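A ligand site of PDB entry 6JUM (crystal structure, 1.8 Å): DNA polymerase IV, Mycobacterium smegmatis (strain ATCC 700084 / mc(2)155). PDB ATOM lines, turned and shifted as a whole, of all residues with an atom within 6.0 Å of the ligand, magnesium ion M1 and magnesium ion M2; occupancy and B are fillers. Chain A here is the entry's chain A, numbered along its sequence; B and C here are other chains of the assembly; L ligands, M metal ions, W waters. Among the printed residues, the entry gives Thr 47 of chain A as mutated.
The guanidinium group of Arg 53 lies within salt-bridge range of an oxygen (O4) of the ligand.
OG1 of Thr 47 is in hydrogen-bond range of O11 of the ligand (2.8 Å).
The backbone NH (N) of Gln 12 is in hydrogen-bond range of an oxygen (O3) of the ligand, at 2.9 Å.
OG1 of Thr 46 is in hydrogen-bond range of O12 of the ligand (3.3 Å).
N4 of the ligand sits at hydrogen-bond distance from O6 of DG 4 of chain C.
A nitrogen (N4) of the ligand is in hydrogen-bond range of N4 of DC 18 of chain B (3.2 Å).
An oxygen (O3) of the ligand is in hydrogen-bond range of the side-chain hydroxyl (OH) of Tyr 50 (2.8 Å).
The side-chain amino group (NZ) of Lys 159 lies within salt-bridge range of an oxygen (O3) of the ligand (3.0 Å).
The backbone NH (N) of Phe 13 lies within hydrogen-bond range of an oxygen (O4) of the ligand.
O of Leu 10 lies close to NZ of Lys 159, at 3.2 Å.
NZ of Lys 159 lies within salt-bridge range of OD1 of Asp 11 (2.8 Å).
The side-chain amide oxygen (OE1) of Gln 12 is in hydrogen-bond range of the backbone NH (N) of Tyr 50 (2.7 Å).
A ring nitrogen (NE2) of His 7 sits at hydrogen-bond distance from the side-chain carboxylate (OE2) of Glu 108.
NZ of Lys 152 is in salt-bridge range of OP1 of DC 18 of chain B, at 2.7 Å.
NE of Arg 53 is in hydrogen-bond range of O of Ala 48.
NZ of Lys 152 is in salt-bridge range of OE2 of Glu 108, at 2.9 Å.
The backbone carbonyl oxygen of Asp 9 sits at hydrogen-bond distance from the side-chain amino group of Lys 159 (3.2 Å).
Asp 11 touches the ligand.
Leu 14 touches the ligand (N to O11, 3.6 Å).
Ala 59 touches the ligand.
CE3 of Trp 106 touches O10 of the ligand, at 3.9 Å.
DG 5 of chain C touches the ligand (N2 to O12, 3.7 Å).
17 residues have an atom within 4 Å of the ligand: Asp 9, Leu 10, Asp 11, Gln 12, Phe 13, Leu 14, Thr 46, Thr 47, Tyr 50, Arg 53, Ala 59, Trp 106, Asp 107, Lys 159, DC 18 of chain B, DG 4 of chain C and DG 5 of chain C.
The nearest printed residue that does not touch the ligand is Glu 108 (4.6 Å).
Lys 159 touches magnesium ion M1 (NZ to MG, 3.9 Å).
Four residues have an atom within 4 Å of magnesium ion M1: Asp 9, Leu 10, Asp 107 and Lys 159.
Along chain A the residues within 4 Å of magnesium ion M1 span positions 9 to 159.
The nearest printed residue that does not touch magnesium ion M1 is Asp 11 (4.5 Å).
Four residues have an atom within 4 Å of magnesium ion M2: Asp 9, Asp 107, Glu 108 and DC 18 of chain B.
The nearest printed residue that does not touch magnesium ion M2 is Lys 152 (4.5 Å).
The side-chain carboxylate (OD2) of Asp 107 is bound to magnesium ion M1, at 2.1 Å.
Magnesium ion M1 is bound by O2 of the ligand (2.2 Å).
Magnesium ion M1 is bound by O7 of the ligand, at 2.2 Å.
Magnesium ion M1 is bound by OD1 of Asp 9, at 2.3 Å.
O5 of the ligand binds magnesium ion M1, 2.3 Å away.
Magnesium ion M1 is bound by O of Leu 10.
The side-chain carboxylate (OD2) of Asp 9 is bound to magnesium ion M2, 2.1 Å away.
OD1 of Asp 107 is bound to magnesium ion M2 (2.2 Å).
Magnesium ion M2 is bound by O7 of the ligand (2.3 Å).
OE1 of Glu 108 binds magnesium ion M2, 2.3 Å away.
O3' of DC 18 of chain B binds magnesium ion M2, 2.3 Å away.
Water W3 is bound to magnesium ion M2 (2.4 Å).
Magnesium ion M2 has six donor atoms within binding distance.
Water W3 lies within hydrogen-bond range of O8 of the ligand (2.8 Å), OP1 of DC 18 of chain B (3.2 Å) and NZ of Lys 152 (3.4 Å).
Water W8 bridges O8 of the ligand and OP2 of DC 18 of chain B.
Water W7 lies within hydrogen-bond range of the backbone carbonyl oxygen of Thr 46 (3.0 Å) and an oxygen (O4) of the ligand (3.2 Å).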
ATOM      1  N   HIS A   7      32.934 -27.094  17.285  1.00  0.00           N
ATOM      2  CA  HIS A   7      31.860 -26.867  16.420  1.00  0.00           C
ATOM      3  C   HIS A   7      32.423 -26.359  15.066  1.00  0.00           C
ATOM      4  O   HIS A   7      33.215 -25.469  15.103  1.00  0.00           O
ATOM      5  CB  HIS A   7      30.970 -25.784  16.913  1.00  0.00           C
ATOM      6  CG  HIS A   7      29.842 -25.477  15.971  1.00  0.00           C
ATOM      7  ND1 HIS A   7      29.834 -24.367  15.177  1.00  0.00           N
ATOM      8  CD2 HIS A   7      28.730 -26.187  15.634  1.00  0.00           C
ATOM      9  CE1 HIS A   7      28.733 -24.340  14.453  1.00  0.00           C
ATOM     10  NE2 HIS A   7      28.045 -25.436  14.686  1.00  0.00           N
ATOM     11  N   ASP A   9      31.930 -25.157  11.109  1.00  0.00           N
ATOM     12  CA  ASP A   9      30.917 -24.470  10.281  1.00  0.00           C
ATOM     13  C   ASP A   9      31.596 -23.947   9.009  1.00  0.00           C
ATOM     14  O   ASP A   9      32.582 -23.244   9.065  1.00  0.00           O
ATOM     15  CB  ASP A   9      30.105 -23.295  10.983  1.00  0.00           C
ATOM     16  CG  ASP A   9      29.009 -22.808  10.148  1.00  0.00           C
ATOM     17  OD1 ASP A   9      29.441 -22.201   9.279  1.00  0.00           O
ATOM     18  OD2 ASP A   9      27.815 -23.012  10.265  1.00  0.00           O
ATOM     19  N   LEU A  10      31.070 -24.471   7.869  1.00  0.00           N
ATOM     20  CA  LEU A  10      31.583 -24.038   6.513  1.00  0.00           C
ATOM     21  C   LEU A  10      31.445 -22.537   6.292  1.00  0.00           C
ATOM     22  O   LEU A  10      30.466 -21.925   6.488  1.00  0.00           O
ATOM     23  CB  LEU A  10      30.876 -24.918   5.415  1.00  0.00           C
ATOM     24  CG  LEU A  10      31.316 -26.404   5.443  1.00  0.00           C
ATOM     25  CD1 LEU A  10      30.447 -27.284   4.582  1.00  0.00           C
ATOM     26  CD2 LEU A  10      32.752 -26.534   4.988  1.00  0.00           C
ATOM     27  N   ASP A  11      32.517 -21.924   5.873  1.00  0.00           N
ATOM     28  CA  ASP A  11      32.505 -20.489   5.491  1.00  0.00           C
ATOM     29  C   ASP A  11      31.748 -20.195   4.226  1.00  0.00           C
ATOM     30  O   ASP A  11      31.911 -20.928   3.182  1.00  0.00           O
ATOM     31  CB  ASP A  11      33.957 -19.945   5.335  1.00  0.00           C
ATOM     32  CG  ASP A  11      34.736 -19.941   6.581  1.00  0.00           C
ATOM     33  OD1 ASP A  11      34.182 -20.328   7.730  1.00  0.00           O
ATOM     34  OD2 ASP A  11      36.000 -19.732   6.447  1.00  0.00           O
ATOM     35  N   GLN A  12      30.919 -19.145   4.315  1.00  0.00           N
ATOM     36  CA  GLN A  12      30.115 -18.736   3.160  1.00  0.00           C
ATOM     37  C   GLN A  12      29.729 -19.929   2.188  1.00  0.00           C
ATOM     38  O   GLN A  12      29.966 -19.883   1.008  1.00  0.00           O
ATOM     39  CB  GLN A  12      30.821 -17.593   2.427  1.00  0.00           C
ATOM     40  CG  GLN A  12      32.264 -17.861   1.973  1.00  0.00           C
ATOM     41  CD  GLN A  12      32.915 -16.702   1.231  1.00  0.00           C
ATOM     42  OE1 GLN A  12      32.324 -15.632   1.032  1.00  0.00           O
ATOM     43  NE2 GLN A  12      34.191 -16.810   1.068  1.00  0.00           N
ATOM     44  N   PHE A  13      29.033 -20.900   2.756  1.00  0.00           N
ATOM     45  CA  PHE A  13      28.991 -22.324   2.140  1.00  0.00           C
ATOM     46  C   PHE A  13      28.707 -22.348   0.672  1.00  0.00           C
ATOM     47  O   PHE A  13      29.554 -22.767  -0.119  1.00  0.00           O
ATOM     48  CB  PHE A  13      27.961 -23.185   2.911  1.00  0.00           C
ATOM     49  CG  PHE A  13      27.778 -24.570   2.402  1.00  0.00           C
ATOM     50  CD1 PHE A  13      28.832 -25.279   1.984  1.00  0.00           C
ATOM     51  CD2 PHE A  13      26.574 -25.159   2.484  1.00  0.00           C
ATOM     52  CE1 PHE A  13      28.702 -26.578   1.459  1.00  0.00           C
ATOM     53  CE2 PHE A  13      26.384 -26.446   1.963  1.00  0.00           C
ATOM     54  CZ  PHE A  13      27.499 -27.174   1.547  1.00  0.00           C
ATOM     55  N   LEU A  14      27.523 -21.907   0.301  1.00  0.00           N
ATOM     56  CA  LEU A  14      27.155 -21.996  -1.134  1.00  0.00           C
ATOM     57  C   LEU A  14      28.086 -21.184  -2.029  1.00  0.00           C
ATOM     58  O   LEU A  14      28.419 -21.678  -3.114  1.00  0.00           O
ATOM     59  CB  LEU A  14      25.734 -21.609  -1.329  1.00  0.00           C
ATOM     60  CG  LEU A  14      24.592 -22.566  -0.939  1.00  0.00           C
ATOM     61  CD1 LEU A  14      24.763 -23.540   0.126  1.00  0.00           C
ATOM     62  CD2 LEU A  14      23.191 -22.036  -0.957  1.00  0.00           C
ATOM     63  N   ALA A  15      28.550 -19.997  -1.588  1.00  0.00           N
ATOM     64  CA  ALA A  15      29.583 -19.219  -2.359  1.00  0.00           C
ATOM     65  C   ALA A  15      30.908 -19.961  -2.499  1.00  0.00           C
ATOM     66  O   ALA A  15      31.496 -19.943  -3.589  1.00  0.00           O
ATOM     67  CB  ALA A  15      29.891 -17.852  -1.807  1.00  0.00           C
ATOM     68  N   VAL A  45      18.506 -13.716  -2.317  1.00  0.00           N
ATOM     69  CA  VAL A  45      19.836 -14.171  -2.028  1.00  0.00           C
ATOM     70  C   VAL A  45      19.754 -15.415  -1.120  1.00  0.00           C
ATOM     71  O   VAL A  45      19.116 -15.377  -0.104  1.00  0.00           O
ATOM     72  CB  VAL A  45      20.660 -13.091  -1.313  1.00  0.00           C
ATOM     73  CG1 VAL A  45      22.036 -13.573  -0.872  1.00  0.00           C
ATOM     74  CG2 VAL A  45      20.829 -11.862  -2.191  1.00  0.00           C
ATOM     75  N   THR A  46      20.370 -16.495  -1.531  1.00  0.00           N
ATOM     76  CA  THR A  46      20.631 -17.617  -0.641  1.00  0.00           C
ATOM     77  C   THR A  46      21.970 -17.505   0.061  1.00  0.00           C
ATOM     78  O   THR A  46      22.022 -17.786   1.235  1.00  0.00           O
ATOM     79  CB  THR A  46      20.413 -19.010  -1.403  1.00  0.00           C
ATOM     80  OG1 THR A  46      20.815 -20.080  -0.521  1.00  0.00           O
ATOM     81  CG2 THR A  46      21.306 -19.170  -2.443  1.00  0.00           C
ATOM     82  N   THR A  47      23.013 -17.106  -0.624  1.00  0.00           N
ATOM     83  CA  THR A  47      24.277 -16.813   0.072  1.00  0.00           C
ATOM     84  C   THR A  47      24.992 -15.650  -0.612  1.00  0.00           C
ATOM     85  O   THR A  47      25.135 -15.640  -1.785  1.00  0.00           O
ATOM     86  CB  THR A  47      25.279 -18.020  -0.005  1.00  0.00           C
ATOM     87  OG1 THR A  47      24.724 -19.238   0.520  1.00  0.00           O
ATOM     88  CG2 THR A  47      26.694 -17.741   0.715  1.00  0.00           C
ATOM     89  N   ALA A  48      25.419 -14.642   0.131  1.00  0.00           N
ATOM     90  CA  ALA A  48      26.342 -13.650  -0.326  1.00  0.00           C
ATOM     91  C   ALA A  48      27.767 -13.978   0.189  1.00  0.00           C
ATOM     92  O   ALA A  48      27.888 -14.428   1.339  1.00  0.00           O
ATOM     93  CB  ALA A  48      25.990 -12.282   0.244  1.00  0.00           C
ATOM     94  N   TYR A  50      31.485 -13.132   1.527  1.00  0.00           N
ATOM     95  CA  TYR A  50      31.834 -12.180   2.554  1.00  0.00           C
ATOM     96  C   TYR A  50      32.044 -10.767   1.921  1.00  0.00           C
ATOM     97  O   TYR A  50      31.800  -9.743   2.611  1.00  0.00           O
ATOM     98  CB  TYR A  50      33.128 -12.611   3.199  1.00  0.00           C
ATOM     99  CG  TYR A  50      33.008 -13.843   4.056  1.00  0.00           C
ATOM    100  CD1 TYR A  50      31.946 -14.102   4.823  1.00  0.00           C
ATOM    101  CD2 TYR A  50      33.986 -14.802   4.030  1.00  0.00           C
ATOM    102  CE1 TYR A  50      31.856 -15.290   5.643  1.00  0.00           C
ATOM    103  CE2 TYR A  50      33.941 -15.892   4.849  1.00  0.00           C
ATOM    104  CZ  TYR A  50      32.863 -16.144   5.628  1.00  0.00           C
ATOM    105  OH  TYR A  50      32.952 -17.285   6.437  1.00  0.00           O
ATOM    106  N   ARG A  53      28.704  -9.182   1.534  1.00  0.00           N
ATOM    107  CA  ARG A  53      28.195  -8.877   2.825  1.00  0.00           C
ATOM    108  C   ARG A  53      28.670  -7.531   3.342  1.00  0.00           C
ATOM    109  O   ARG A  53      27.957  -6.876   4.083  1.00  0.00           O
ATOM    110  CB  ARG A  53      28.600  -9.924   3.897  1.00  0.00           C
ATOM    111  CG  ARG A  53      27.910 -11.240   3.652  1.00  0.00           C
ATOM    112  CD  ARG A  53      28.192 -12.412   4.693  1.00  0.00           C
ATOM    113  NE  ARG A  53      27.962 -13.674   4.061  1.00  0.00           N
ATOM    114  CZ  ARG A  53      27.951 -14.816   4.767  1.00  0.00           C
ATOM    115  NH1 ARG A  53      28.222 -14.843   6.033  1.00  0.00           N
ATOM    116  NH2 ARG A  53      27.735 -15.929   4.154  1.00  0.00           N
ATOM    117  N   ALA A  59      21.527 -13.190   3.221  1.00  0.00           N
ATOM    118  CA  ALA A  59      20.557 -14.223   2.834  1.00  0.00           C
ATOM    119  C   ALA A  59      19.125 -13.640   3.081  1.00  0.00           C
ATOM    120  O   ALA A  59      18.900 -12.958   4.061  1.00  0.00           O
ATOM    121  CB  ALA A  59      20.765 -15.510   3.716  1.00  0.00           C
ATOM    122  N   GLY A  60      18.181 -13.929   2.204  1.00  0.00           N
ATOM    123  CA  GLY A  60      16.806 -13.380   2.257  1.00  0.00           C
ATOM    124  C   GLY A  60      16.519 -12.131   1.498  1.00  0.00           C
ATOM    125  O   GLY A  60      15.375 -11.739   1.319  1.00  0.00           O
ATOM    126  N   TRP A 106      23.023 -28.906   7.206  1.00  0.00           N
ATOM    127  CA  TRP A 106      23.784 -28.994   6.033  1.00  0.00           C
ATOM    128  C   TRP A 106      25.277 -28.700   6.077  1.00  0.00           C
ATOM    129  O   TRP A 106      26.097 -29.303   5.355  1.00  0.00           O
ATOM    130  CB  TRP A 106      23.080 -27.859   5.233  1.00  0.00           C
ATOM    131  CG  TRP A 106      23.043 -28.148   3.907  1.00  0.00           C
ATOM    132  CD1 TRP A 106      23.330 -29.301   3.290  1.00  0.00           C
ATOM    133  CD2 TRP A 106      22.649 -27.228   2.951  1.00  0.00           C
ATOM    134  NE1 TRP A 106      23.153 -29.136   1.897  1.00  0.00           N
ATOM    135  CE2 TRP A 106      22.729 -27.868   1.674  1.00  0.00           C
ATOM    136  CE3 TRP A 106      22.282 -25.900   3.013  1.00  0.00           C
ATOM    137  CZ2 TRP A 106      22.395 -27.221   0.492  1.00  0.00           C
ATOM    138  CZ3 TRP A 106      21.950 -25.263   1.821  1.00  0.00           C
ATOM    139  CH2 TRP A 106      22.028 -25.912   0.581  1.00  0.00           C
ATOM    140  N   ASP A 107      25.640 -27.712   6.851  1.00  0.00           N
ATOM    141  CA  ASP A 107      26.997 -27.128   6.757  1.00  0.00           C
ATOM    142  C   ASP A 107      27.781 -27.093   8.109  1.00  0.00           C
ATOM    143  O   ASP A 107      28.862 -26.491   8.235  1.00  0.00           O
ATOM    144  CB  ASP A 107      26.940 -25.730   6.062  1.00  0.00           C
ATOM    145  CG  ASP A 107      27.047 -24.507   6.998  1.00  0.00           C
ATOM    146  OD1 ASP A 107      26.303 -24.530   7.985  1.00  0.00           O
ATOM    147  OD2 ASP A 107      27.832 -23.611   6.741  1.00  0.00           O
ATOM    148  N   GLU A 108      27.286 -27.836   9.126  1.00  0.00           N
ATOM    149  CA  GLU A 108      27.981 -27.785  10.362  1.00  0.00           C
ATOM    150  C   GLU A 108      27.893 -29.080  11.125  1.00  0.00           C
ATOM    151  O   GLU A 108      26.930 -29.876  10.915  1.00  0.00           O
ATOM    152  CB  GLU A 108      27.531 -26.653  11.224  1.00  0.00           C
ATOM    153  CG  GLU A 108      26.067 -26.491  11.496  1.00  0.00           C
ATOM    154  CD  GLU A 108      25.738 -25.112  12.040  1.00  0.00           C
ATOM    155  OE1 GLU A 108      25.165 -24.302  11.343  1.00  0.00           O
ATOM    156  OE2 GLU A 108      25.699 -24.992  13.284  1.00  0.00           O
ATOM    157  N   LYS A 152      29.284 -23.241  19.694  1.00  0.00           N
ATOM    158  CA  LYS A 152      28.606 -22.559  18.608  1.00  0.00           C
ATOM    159  C   LYS A 152      28.758 -21.063  18.689  1.00  0.00           C
ATOM    160  O   LYS A 152      29.041 -20.440  17.632  1.00  0.00           O
ATOM    161  CB  LYS A 152      27.091 -22.956  18.627  1.00  0.00           C
ATOM    162  CG  LYS A 152      26.200 -22.193  17.673  1.00  0.00           C
ATOM    163  CD  LYS A 152      26.474 -22.483  16.208  1.00  0.00           C
ATOM    164  CE  LYS A 152      25.173 -22.113  15.454  1.00  0.00           C
ATOM    165  NZ  LYS A 152      25.497 -22.206  13.958  1.00  0.00           N
ATOM    166  N   LYS A 159      34.969 -16.908  12.886  1.00  0.00           N
ATOM    167  CA  LYS A 159      34.768 -16.525  11.495  1.00  0.00           C
ATOM    168  C   LYS A 159      35.526 -15.236  11.158  1.00  0.00           C
ATOM    169  O   LYS A 159      35.508 -14.352  12.028  1.00  0.00           O
ATOM    170  CB  LYS A 159      33.325 -16.207  11.293  1.00  0.00           C
ATOM    171  CG  LYS A 159      32.395 -17.384  11.296  1.00  0.00           C
ATOM    172  CD  LYS A 159      32.604 -18.382  10.238  1.00  0.00           C
ATOM    173  CE  LYS A 159      31.504 -19.485  10.228  1.00  0.00           C
ATOM    174  NZ  LYS A 159      31.634 -20.187   8.897  1.00  0.00           N
ATOM    175  P    DC B  18      21.931 -20.499  12.738  1.00  0.00           P
ATOM    176  OP1  DC B  18      23.302 -20.738  13.322  1.00  0.00           O
ATOM    177  OP2  DC B  18      21.717 -19.097  12.315  1.00  0.00           O
ATOM    178  O5'  DC B  18      21.623 -21.386  11.494  1.00  0.00           O
ATOM    179  C5'  DC B  18      21.867 -22.752  11.554  1.00  0.00           C
ATOM    180  C4'  DC B  18      21.686 -23.347  10.188  1.00  0.00           C
ATOM    181  O4'  DC B  18      20.283 -23.325   9.865  1.00  0.00           O
ATOM    182  C3'  DC B  18      22.381 -22.671   9.017  1.00  0.00           C
ATOM    183  O3'  DC B  18      23.646 -23.303   8.745  1.00  0.00           O
ATOM    184  C2'  DC B  18      21.495 -23.056   7.849  1.00  0.00           C
ATOM    185  C1'  DC B  18      20.116 -23.037   8.466  1.00  0.00           C
ATOM    186  N1   DC B  18      19.236 -21.817   8.302  1.00  0.00           N
ATOM    187  C2   DC B  18      18.348 -21.836   7.214  1.00  0.00           C
ATOM    188  O2   DC B  18      18.475 -22.735   6.366  1.00  0.00           O
ATOM    189  N3   DC B  18      17.434 -20.847   7.085  1.00  0.00           N
ATOM    190  C4   DC B  18      17.360 -19.886   7.996  1.00  0.00           C
ATOM    191  N4   DC B  18      16.421 -18.942   7.828  1.00  0.00           N
ATOM    192  C5   DC B  18      18.252 -19.833   9.120  1.00  0.00           C
ATOM    193  C6   DC B  18      19.147 -20.831   9.247  1.00  0.00           C
ATOM    194  P    DG C   4       9.543 -13.910  -0.447  1.00  0.00           P
ATOM    195  OP1  DG C   4       8.357 -13.893  -1.350  1.00  0.00           O
ATOM    196  OP2  DG C   4       9.385 -14.321   0.992  1.00  0.00           O
ATOM    197  O5'  DG C   4      10.614 -14.900  -1.039  1.00  0.00           O
ATOM    198  C5'  DG C   4      10.930 -15.033  -2.424  1.00  0.00           C
ATOM    199  C4'  DG C   4      11.468 -16.422  -2.627  1.00  0.00           C
ATOM    200  O4'  DG C   4      12.735 -16.606  -1.949  1.00  0.00           O
ATOM    201  C3'  DG C   4      10.535 -17.565  -2.149  1.00  0.00           C
ATOM    202  O3'  DG C   4      10.580 -18.650  -3.093  1.00  0.00           O
ATOM    203  C2'  DG C   4      11.098 -17.926  -0.799  1.00  0.00           C
ATOM    204  C1'  DG C   4      12.616 -17.620  -0.946  1.00  0.00           C
ATOM    205  N9   DG C   4      13.268 -17.138   0.270  1.00  0.00           N
ATOM    206  C8   DG C   4      12.861 -16.105   1.072  1.00  0.00           C
ATOM    207  N7   DG C   4      13.660 -15.884   2.076  1.00  0.00           N
ATOM    208  C5   DG C   4      14.621 -16.872   1.979  1.00  0.00           C
ATOM    209  C6   DG C   4      15.746 -17.159   2.807  1.00  0.00           C
ATOM    210  O6   DG C   4      16.146 -16.538   3.793  1.00  0.00           O
ATOM    211  N1   DG C   4      16.493 -18.219   2.312  1.00  0.00           N
ATOM    212  C2   DG C   4      16.152 -18.976   1.206  1.00  0.00           C
ATOM    213  N2   DG C   4      16.949 -19.990   0.910  1.00  0.00           N
ATOM    214  N3   DG C   4      15.092 -18.722   0.440  1.00  0.00           N
ATOM    215  C4   DG C   4      14.373 -17.686   0.884  1.00  0.00           C
ATOM    216  P    DG C   5       9.670 -19.976  -2.820  1.00  0.00           P
ATOM    217  OP1  DG C   5       9.511 -20.578  -4.139  1.00  0.00           O
ATOM    218  OP2  DG C   5       8.632 -19.711  -1.828  1.00  0.00           O
ATOM    219  O5'  DG C   5      10.659 -20.854  -1.917  1.00  0.00           O
ATOM    220  C5'  DG C   5      11.817 -21.394  -2.566  1.00  0.00           C
ATOM    221  C4'  DG C   5      12.499 -22.317  -1.577  1.00  0.00           C
ATOM    222  O4'  DG C   5      13.065 -21.528  -0.483  1.00  0.00           O
ATOM    223  C3'  DG C   5      11.567 -23.364  -0.919  1.00  0.00           C
ATOM    224  O3'  DG C   5      12.232 -24.637  -0.951  1.00  0.00           O
ATOM    225  C2'  DG C   5      11.441 -22.891   0.526  1.00  0.00           C
ATOM    226  C1'  DG C   5      12.807 -22.254   0.727  1.00  0.00           C
ATOM    227  N9   DG C   5      12.929 -21.315   1.834  1.00  0.00           N
ATOM    228  C8   DG C   5      12.109 -20.255   2.143  1.00  0.00           C
ATOM    229  N7   DG C   5      12.525 -19.559   3.157  1.00  0.00           N
ATOM    230  C5   DG C   5      13.653 -20.249   3.596  1.00  0.00           C
ATOM    231  C6   DG C   5      14.533 -19.989   4.675  1.00  0.00           C
ATOM    232  O6   DG C   5      14.446 -19.101   5.527  1.00  0.00           O
ATOM    233  N1   DG C   5      15.558 -20.918   4.740  1.00  0.00           N
ATOM    234  C2   DG C   5      15.752 -21.949   3.863  1.00  0.00           C
ATOM    235  N2   DG C   5      16.829 -22.755   4.088  1.00  0.00           N
ATOM    236  N3   DG C   5      14.932 -22.208   2.854  1.00  0.00           N
ATOM    237  C4   DG C   5      13.948 -21.292   2.746  1.00  0.00           C
HETATM  238  P1  LIG L   1      29.061 -18.352   7.443  1.00  0.00           P
HETATM  239  O1  LIG L   1      28.770 -17.048   8.104  1.00  0.00           O
HETATM  240  O2  LIG L   1      28.548 -19.595   8.213  1.00  0.00           O
HETATM  241  O3  LIG L   1      30.437 -18.239   7.030  1.00  0.00           O
HETATM  242  P2  LIG L   1      27.071 -19.340   5.508  1.00  0.00           P
HETATM  243  O4  LIG L   1      26.807 -18.727   4.114  1.00  0.00           O
HETATM  244  O5  LIG L   1      27.677 -20.651   5.410  1.00  0.00           O
HETATM  245  O6  LIG L   1      28.100 -18.337   6.099  1.00  0.00           O
HETATM  246  P3  LIG L   1      25.173 -20.446   7.553  1.00  0.00           P
HETATM  247  O7  LIG L   1      26.172 -21.470   7.902  1.00  0.00           O
HETATM  248  O8  LIG L   1      24.231 -19.776   8.540  1.00  0.00           O
HETATM  249  N1  LIG L   1      25.842 -19.310   6.613  1.00  0.00           N
HETATM  250  O9  LIG L   1      24.086 -21.236   6.728  1.00  0.00           O
HETATM  251  C1  LIG L   1      24.519 -22.144   5.690  1.00  0.00           C
HETATM  252  C2  LIG L   1      23.867 -22.068   4.304  1.00  0.00           C
HETATM  253  O10 LIG L   1      22.439 -22.325   4.566  1.00  0.00           O
HETATM  254  C3  LIG L   1      24.001 -20.864   3.578  1.00  0.00           C
HETATM  255  O11 LIG L   1      25.270 -20.662   2.859  1.00  0.00           O
HETATM  256  C4  LIG L   1      22.678 -21.041   2.650  1.00  0.00           C
HETATM  257  C5  LIG L   1      21.674 -21.616   3.478  1.00  0.00           C
HETATM  258  N2  LIG L   1      20.866 -20.611   4.162  1.00  0.00           N
HETATM  259  C6  LIG L   1      19.573 -20.214   3.404  1.00  0.00           C
HETATM  260  N3  LIG L   1      18.759 -19.172   3.978  1.00  0.00           N
HETATM  261  C7  LIG L   1      19.099 -18.527   5.176  1.00  0.00           C
HETATM  262  C8  LIG L   1      20.378 -18.881   5.894  1.00  0.00           C
HETATM  263  C9  LIG L   1      21.198 -19.980   5.392  1.00  0.00           C
HETATM  264  O12 LIG L   1      19.346 -20.779   2.314  1.00  0.00           O
HETATM  265  N4  LIG L   1      18.302 -17.496   5.627  1.00  0.00           N
HETATM  266 MG    MG M   1      28.327 -21.637   7.370  1.00  0.00          MG
HETATM  267 MG    MG M   2      25.811 -23.024   9.538  1.00  0.00          MG
HETATM  268  O   HOH W   1      19.240 -23.056   1.042  1.00  0.00           O
HETATM  269  O   HOH W   2      30.317 -15.023   9.241  1.00  0.00           O
HETATM  270  O   HOH W   3      25.178 -21.078  10.797  1.00  0.00           O
HETATM  271  O   HOH W   4      19.008 -15.806   8.037  1.00  0.00           O
HETATM  272  O   HOH W   5      23.720 -17.253   6.241  1.00  0.00           O
HETATM  273  O   HOH W   6      27.453 -19.622  10.601  1.00  0.00           O
HETATM  274  O   HOH W   7      23.873 -17.510   3.554  1.00  0.00           O
HETATM  275  O   HOH W   8      21.724 -18.580   9.214  1.00  0.00           O
